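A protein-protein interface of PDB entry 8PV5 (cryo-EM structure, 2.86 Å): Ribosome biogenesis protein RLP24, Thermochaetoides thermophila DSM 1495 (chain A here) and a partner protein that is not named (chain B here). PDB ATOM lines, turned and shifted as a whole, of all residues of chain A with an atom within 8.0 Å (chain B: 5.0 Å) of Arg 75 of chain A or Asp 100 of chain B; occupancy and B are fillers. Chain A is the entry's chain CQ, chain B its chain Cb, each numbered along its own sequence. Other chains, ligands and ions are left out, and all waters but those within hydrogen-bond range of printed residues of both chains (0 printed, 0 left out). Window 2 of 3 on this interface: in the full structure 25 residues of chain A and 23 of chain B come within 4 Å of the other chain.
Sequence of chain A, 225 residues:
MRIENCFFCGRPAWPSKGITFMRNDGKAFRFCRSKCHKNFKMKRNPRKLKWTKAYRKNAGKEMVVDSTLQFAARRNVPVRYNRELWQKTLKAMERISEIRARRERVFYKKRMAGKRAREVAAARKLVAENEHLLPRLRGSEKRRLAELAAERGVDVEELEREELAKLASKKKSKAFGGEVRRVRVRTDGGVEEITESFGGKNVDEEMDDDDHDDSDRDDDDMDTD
Ala 72 of chain A touches Arg 98 of chain B (O to CG, 3.2 Å). Ala 73 of chain A touches Arg 98 of chain B (CA to O, 3.3 Å). CB of Ala 73 of chain A touches CB of Asp 100 of chain B (3.7 Å). Asn 76 of chain A touches Ile 99 of chain B.
Printed residues of chain A that touch a printed residue of chain B: Gln 70, Ala 72, Ala 73, Arg 74, Arg 75 and Asn 76. Hydrophobic or aromatic side chains of chain A within 4 Å of the printed part of chain B: Ala 73. Printed residues of chain B that touch a printed residue of chain A: Arg 98, Ile 99, Asp 100 and Asn 101. Among the printed residues, Asp or Glu carboxylates within 4 Å of a Lys or Arg side-chain nitrogen of the other chain: Arg 75 of chain A with Asp 100 of chain B (3.4 Å).
The guanidinium group (NH2) of Arg 98 of chain B is in hydrogen-bond range of the backbone carbonyl oxygen (O) of Gln 70 of chain A (2.8 Å). The backbone carbonyl oxygen of Arg 98 of chain B lies within hydrogen-bond range of the backbone NH of Arg 74 of chain A, at 2.8 Å. The backbone NH (N) of Asp 100 of chain B is in hydrogen-bond range of the backbone carbonyl oxygen (O) of Arg 74 of chain A (3.1 Å). NH1 of Arg 75 of chain A lies within salt-bridge range of OD1 of Asp 100 of chain B, 3.4 Å away. N of Asn 76 of chain A is in hydrogen-bond range of O of Asp 100 of chain B, at 3.2 Å. The side-chain amide nitrogen (ND2) of Asn 76 of chain A is in hydrogen-bond range of the side-chain amide oxygen (OD1) of Asn 101 of chain B, at 2.5 Å.
Of chain B, only Asp 100 comes within 4 Å of Arg 75 of chain A. Asp 100 of chain B touches four residues of chain A. Printed residues of chain A within 4 Å of Ile 99 of chain B: Asn 76 (3.6 Å). Printed residues of chain B within 4 Å of Asn 76 of chain A: Ile 99 (3.6 Å), Asp 100 (3.2 Å) and Asn 101 (2.5 Å). Printed residues of chain B within 4 Å of Gln 70 of chain A: Arg 98 (2.8 Å). Of the printed residues of chain B, Arg 74 of chain A touches Arg 98 and Asp 100. Of the printed residues of chain A, Asn 101 of chain B touches Asn 76. The nearest residue of chain B that does not touch Arg 75 of chain A is Arg 98 of chain B (4.5 Å). The nearest printed residue of chain B that does not touch Ala 73 of chain A is Ile 99 of chain B (4.8 Å).
The backbone carbonyl oxygen of Phe 71 of chain A lies within hydrogen-bond range of the guanidinium group of Arg 75 of chain A (3.1 Å). NH1 of Arg 98 of chain B is in salt-bridge range of OD2 of Asp 100 of chain B (3.4 Å).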
ATOM      1  N   ARG A   2       0.307   0.729  -1.218  1.00  0.00           N
ATOM      2  CA  ARG A   2       1.502   1.142  -0.500  1.00  0.00           C
ATOM      3  C   ARG A   2       1.164   2.353   0.356  1.00  0.00           C
ATOM      4  O   ARG A   2       0.104   2.963   0.213  1.00  0.00           O
ATOM      5  CB  ARG A   2       2.661   1.470  -1.450  1.00  0.00           C
ATOM      6  CG  ARG A   2       2.448   2.713  -2.287  1.00  0.00           C
ATOM      7  CD  ARG A   2       3.734   3.147  -2.969  1.00  0.00           C
ATOM      8  NE  ARG A   2       4.689   3.728  -2.033  1.00  0.00           N
ATOM      9  CZ  ARG A   2       5.772   3.108  -1.583  1.00  0.00           C
ATOM     10  NH1 ARG A   2       6.075   1.880  -1.969  1.00  0.00           N
ATOM     11  NH2 ARG A   2       6.572   3.738  -0.727  1.00  0.00           N
ATOM     12  N   GLN A  70      18.879   3.857   6.591  1.00  0.00           N
ATOM     13  CA  GLN A  70      19.303   3.568   5.228  1.00  0.00           C
ATOM     14  C   GLN A  70      18.587   2.372   4.619  1.00  0.00           C
ATOM     15  O   GLN A  70      18.771   2.098   3.430  1.00  0.00           O
ATOM     16  CB  GLN A  70      20.817   3.335   5.187  1.00  0.00           C
ATOM     17  CG  GLN A  70      21.641   4.559   5.541  1.00  0.00           C
ATOM     18  CD  GLN A  70      21.432   5.701   4.568  1.00  0.00           C
ATOM     19  OE1 GLN A  70      20.821   6.714   4.905  1.00  0.00           O
ATOM     20  NE2 GLN A  70      21.940   5.541   3.352  1.00  0.00           N
ATOM     21  N   PHE A  71      17.779   1.657   5.397  1.00  0.00           N
ATOM     22  CA  PHE A  71      17.054   0.503   4.885  1.00  0.00           C
ATOM     23  C   PHE A  71      15.808   0.884   4.101  1.00  0.00           C
ATOM     24  O   PHE A  71      15.282   0.049   3.357  1.00  0.00           O
ATOM     25  CB  PHE A  71      16.663  -0.424   6.039  1.00  0.00           C
ATOM     26  CG  PHE A  71      17.834  -1.074   6.716  1.00  0.00           C
ATOM     27  CD1 PHE A  71      18.318  -2.294   6.273  1.00  0.00           C
ATOM     28  CD2 PHE A  71      18.451  -0.467   7.798  1.00  0.00           C
ATOM     29  CE1 PHE A  71      19.395  -2.896   6.897  1.00  0.00           C
ATOM     30  CE2 PHE A  71      19.530  -1.062   8.424  1.00  0.00           C
ATOM     31  CZ  PHE A  71      20.001  -2.279   7.973  1.00  0.00           C
ATOM     32  N   ALA A  72      15.337   2.119   4.234  1.00  0.00           N
ATOM     33  CA  ALA A  72      14.148   2.596   3.541  1.00  0.00           C
ATOM     34  C   ALA A  72      14.547   3.194   2.205  1.00  0.00           C
ATOM     35  O   ALA A  72      15.297   4.174   2.160  1.00  0.00           O
ATOM     36  CB  ALA A  72      13.401   3.632   4.382  1.00  0.00           C
ATOM     37  N   ALA A  73      14.044   2.607   1.123  1.00  0.00           N
ATOM     38  CA  ALA A  73      14.323   3.115  -0.209  1.00  0.00           C
ATOM     39  C   ALA A  73      13.170   2.755  -1.130  1.00  0.00           C
ATOM     40  O   ALA A  73      12.404   1.825  -0.869  1.00  0.00           O
ATOM     41  CB  ALA A  73      15.640   2.560  -0.761  1.00  0.00           C
ATOM     42  N   ARG A  74      13.053   3.514  -2.215  1.00  0.00           N
ATOM     43  CA  ARG A  74      12.113   3.190  -3.280  1.00  0.00           C
ATOM     44  C   ARG A  74      12.812   2.241  -4.243  1.00  0.00           C
ATOM     45  O   ARG A  74      13.617   2.669  -5.076  1.00  0.00           O
ATOM     46  CB  ARG A  74      11.637   4.458  -3.980  1.00  0.00           C
ATOM     47  CG  ARG A  74      10.707   4.217  -5.156  1.00  0.00           C
ATOM     48  CD  ARG A  74      10.393   5.523  -5.878  1.00  0.00           C
ATOM     49  NE  ARG A  74       9.353   5.392  -6.894  1.00  0.00           N
ATOM     50  CZ  ARG A  74       8.064   5.179  -6.651  1.00  0.00           C
ATOM     51  NH1 ARG A  74       7.589   5.110  -5.419  1.00  0.00           N
ATOM     52  NH2 ARG A  74       7.227   5.049  -7.677  1.00  0.00           N
ATOM     53  N   ARG A  75      12.521   0.949  -4.116  1.00  0.00           N
ATOM     54  CA  ARG A  75      13.206  -0.081  -4.888  1.00  0.00           C
ATOM     55  C   ARG A  75      12.667  -0.061  -6.312  1.00  0.00           C
ATOM     56  O   ARG A  75      11.540  -0.495  -6.565  1.00  0.00           O
ATOM     57  CB  ARG A  75      13.018  -1.452  -4.246  1.00  0.00           C
ATOM     58  CG  ARG A  75      13.266  -1.464  -2.751  1.00  0.00           C
ATOM     59  CD  ARG A  75      14.745  -1.385  -2.429  1.00  0.00           C
ATOM     60  NE  ARG A  75      14.982  -1.412  -0.992  1.00  0.00           N
ATOM     61  CZ  ARG A  75      16.182  -1.468  -0.432  1.00  0.00           C
ATOM     62  NH1 ARG A  75      17.283  -1.503  -1.162  1.00  0.00           N
ATOM     63  NH2 ARG A  75      16.279  -1.490   0.893  1.00  0.00           N
ATOM     64  N   ASN A  76      13.474   0.448  -7.238  1.00  0.00           N
ATOM     65  CA  ASN A  76      13.099   0.529  -8.639  1.00  0.00           C
ATOM     66  C   ASN A  76      13.525  -0.691  -9.442  1.00  0.00           C
ATOM     67  O   ASN A  76      13.162  -0.795 -10.619  1.00  0.00           O
ATOM     68  CB  ASN A  76      13.696   1.793  -9.265  1.00  0.00           C
ATOM     69  CG  ASN A  76      12.905   3.038  -8.923  1.00  0.00           C
ATOM     70  OD1 ASN A  76      11.743   2.960  -8.526  1.00  0.00           O
ATOM     71  ND2 ASN A  76      13.529   4.197  -9.079  1.00  0.00           N
ATOM     72  N   VAL A  77      14.280  -1.606  -8.843  1.00  0.00           N
ATOM     73  CA  VAL A  77      14.643  -2.868  -9.482  1.00  0.00           C
ATOM     74  C   VAL A  77      13.947  -3.997  -8.732  1.00  0.00           C
ATOM     75  O   VAL A  77      14.315  -4.292  -7.586  1.00  0.00           O
ATOM     76  CB  VAL A  77      16.165  -3.071  -9.508  1.00  0.00           C
ATOM     77  CG1 VAL A  77      16.508  -4.389 -10.183  1.00  0.00           C
ATOM     78  CG2 VAL A  77      16.840  -1.915 -10.215  1.00  0.00           C
ATOM     79  N   PRO A  78      12.939  -4.639  -9.321  1.00  0.00           N
ATOM     80  CA  PRO A  78      12.217  -5.696  -8.605  1.00  0.00           C
ATOM     81  C   PRO A  78      13.061  -6.949  -8.418  1.00  0.00           C
ATOM     82  O   PRO A  78      13.976  -7.237  -9.193  1.00  0.00           O
ATOM     83  CB  PRO A  78      11.008  -5.966  -9.504  1.00  0.00           C
ATOM     84  CG  PRO A  78      11.454  -5.544 -10.856  1.00  0.00           C
ATOM     85  CD  PRO A  78      12.336  -4.357 -10.634  1.00  0.00           C
ATOM     86  N   VAL A  79      12.734  -7.697  -7.367  1.00  0.00           N
ATOM     87  CA  VAL A  79      13.420  -8.929  -7.001  1.00  0.00           C
ATOM     88  C   VAL A  79      12.416 -10.072  -7.084  1.00  0.00           C
ATOM     89  O   VAL A  79      11.246  -9.908  -6.715  1.00  0.00           O
ATOM     90  CB  VAL A  79      14.039  -8.818  -5.591  1.00  0.00           C
ATOM     91  CG1 VAL A  79      14.781 -10.088  -5.202  1.00  0.00           C
ATOM     92  CG2 VAL A  79      14.974  -7.621  -5.517  1.00  0.00           C
ATOM     93  N   ARG B  98      14.579   7.497   0.418  1.00  0.00           N
ATOM     94  CA  ARG B  98      15.515   7.673  -0.684  1.00  0.00           C
ATOM     95  C   ARG B  98      15.074   6.815  -1.861  1.00  0.00           C
ATOM     96  O   ARG B  98      14.125   6.034  -1.771  1.00  0.00           O
ATOM     97  CB  ARG B  98      16.951   7.328  -0.270  1.00  0.00           C
ATOM     98  CG  ARG B  98      17.159   5.879   0.117  1.00  0.00           C
ATOM     99  CD  ARG B  98      18.588   5.620   0.554  1.00  0.00           C
ATOM    100  NE  ARG B  98      18.781   4.243   0.989  1.00  0.00           N
ATOM    101  CZ  ARG B  98      19.148   3.249   0.192  1.00  0.00           C
ATOM    102  NH1 ARG B  98      19.380   3.447  -1.095  1.00  0.00           N
ATOM    103  NH2 ARG B  98      19.284   2.028   0.699  1.00  0.00           N
ATOM    104  N   ILE B  99      15.774   6.975  -2.980  1.00  0.00           N
ATOM    105  CA  ILE B  99      15.486   6.246  -4.208  1.00  0.00           C
ATOM    106  C   ILE B  99      16.670   5.340  -4.512  1.00  0.00           C
ATOM    107  O   ILE B  99      17.802   5.816  -4.664  1.00  0.00           O
ATOM    108  CB  ILE B  99      15.205   7.197  -5.381  1.00  0.00           C
ATOM    109  CG1 ILE B  99      13.958   8.034  -5.101  1.00  0.00           C
ATOM    110  CG2 ILE B  99      15.041   6.417  -6.672  1.00  0.00           C
ATOM    111  CD1 ILE B  99      13.759   9.169  -6.078  1.00  0.00           C
ATOM    112  N   ASP B 100      16.410   4.039  -4.603  1.00  0.00           N
ATOM    113  CA  ASP B 100      17.423   3.053  -4.950  1.00  0.00           C
ATOM    114  C   ASP B 100      17.199   2.604  -6.388  1.00  0.00           C
ATOM    115  O   ASP B 100      16.167   2.003  -6.701  1.00  0.00           O
ATOM    116  CB  ASP B 100      17.373   1.859  -3.999  1.00  0.00           C
ATOM    117  CG  ASP B 100      18.660   1.061  -3.999  1.00  0.00           C
ATOM    118  OD1 ASP B 100      18.587  -0.186  -4.009  1.00  0.00           O
ATOM    119  OD2 ASP B 100      19.745   1.680  -3.992  1.00  0.00           O
ATOM    120  N   ASN B 101      18.165   2.899  -7.258  1.00  0.00           N
ATOM    121  CA  ASN B 101      18.078   2.558  -8.671  1.00  0.00           C
ATOM    122  C   ASN B 101      19.067   1.467  -9.063  1.00  0.00           C
ATOM    123  O   ASN B 101      19.311   1.254 -10.255  1.00  0.00           O
ATOM    124  CB  ASN B 101      18.298   3.806  -9.526  1.00  0.00           C
ATOM    125  CG  ASN B 101      17.146   4.784  -9.435  1.00  0.00           C
ATOM    126  OD1 ASN B 101      15.996   4.391  -9.250  1.00  0.00           O
ATOM    127  ND2 ASN B 101      17.450   6.069  -9.560  1.00  0.00           N
ATOM    128  N   GLY B 102      19.640   0.772  -8.086  1.00  0.00           N
ATOM    129  CA  GLY B 102      20.600  -0.280  -8.360  1.00  0.00           C
ATOM    130  C   GLY B 102      22.032   0.215  -8.396  1.00  0.00           C
ATOM    131  O   GLY B 102      22.899  -0.310  -7.697  1.00  0.00           O
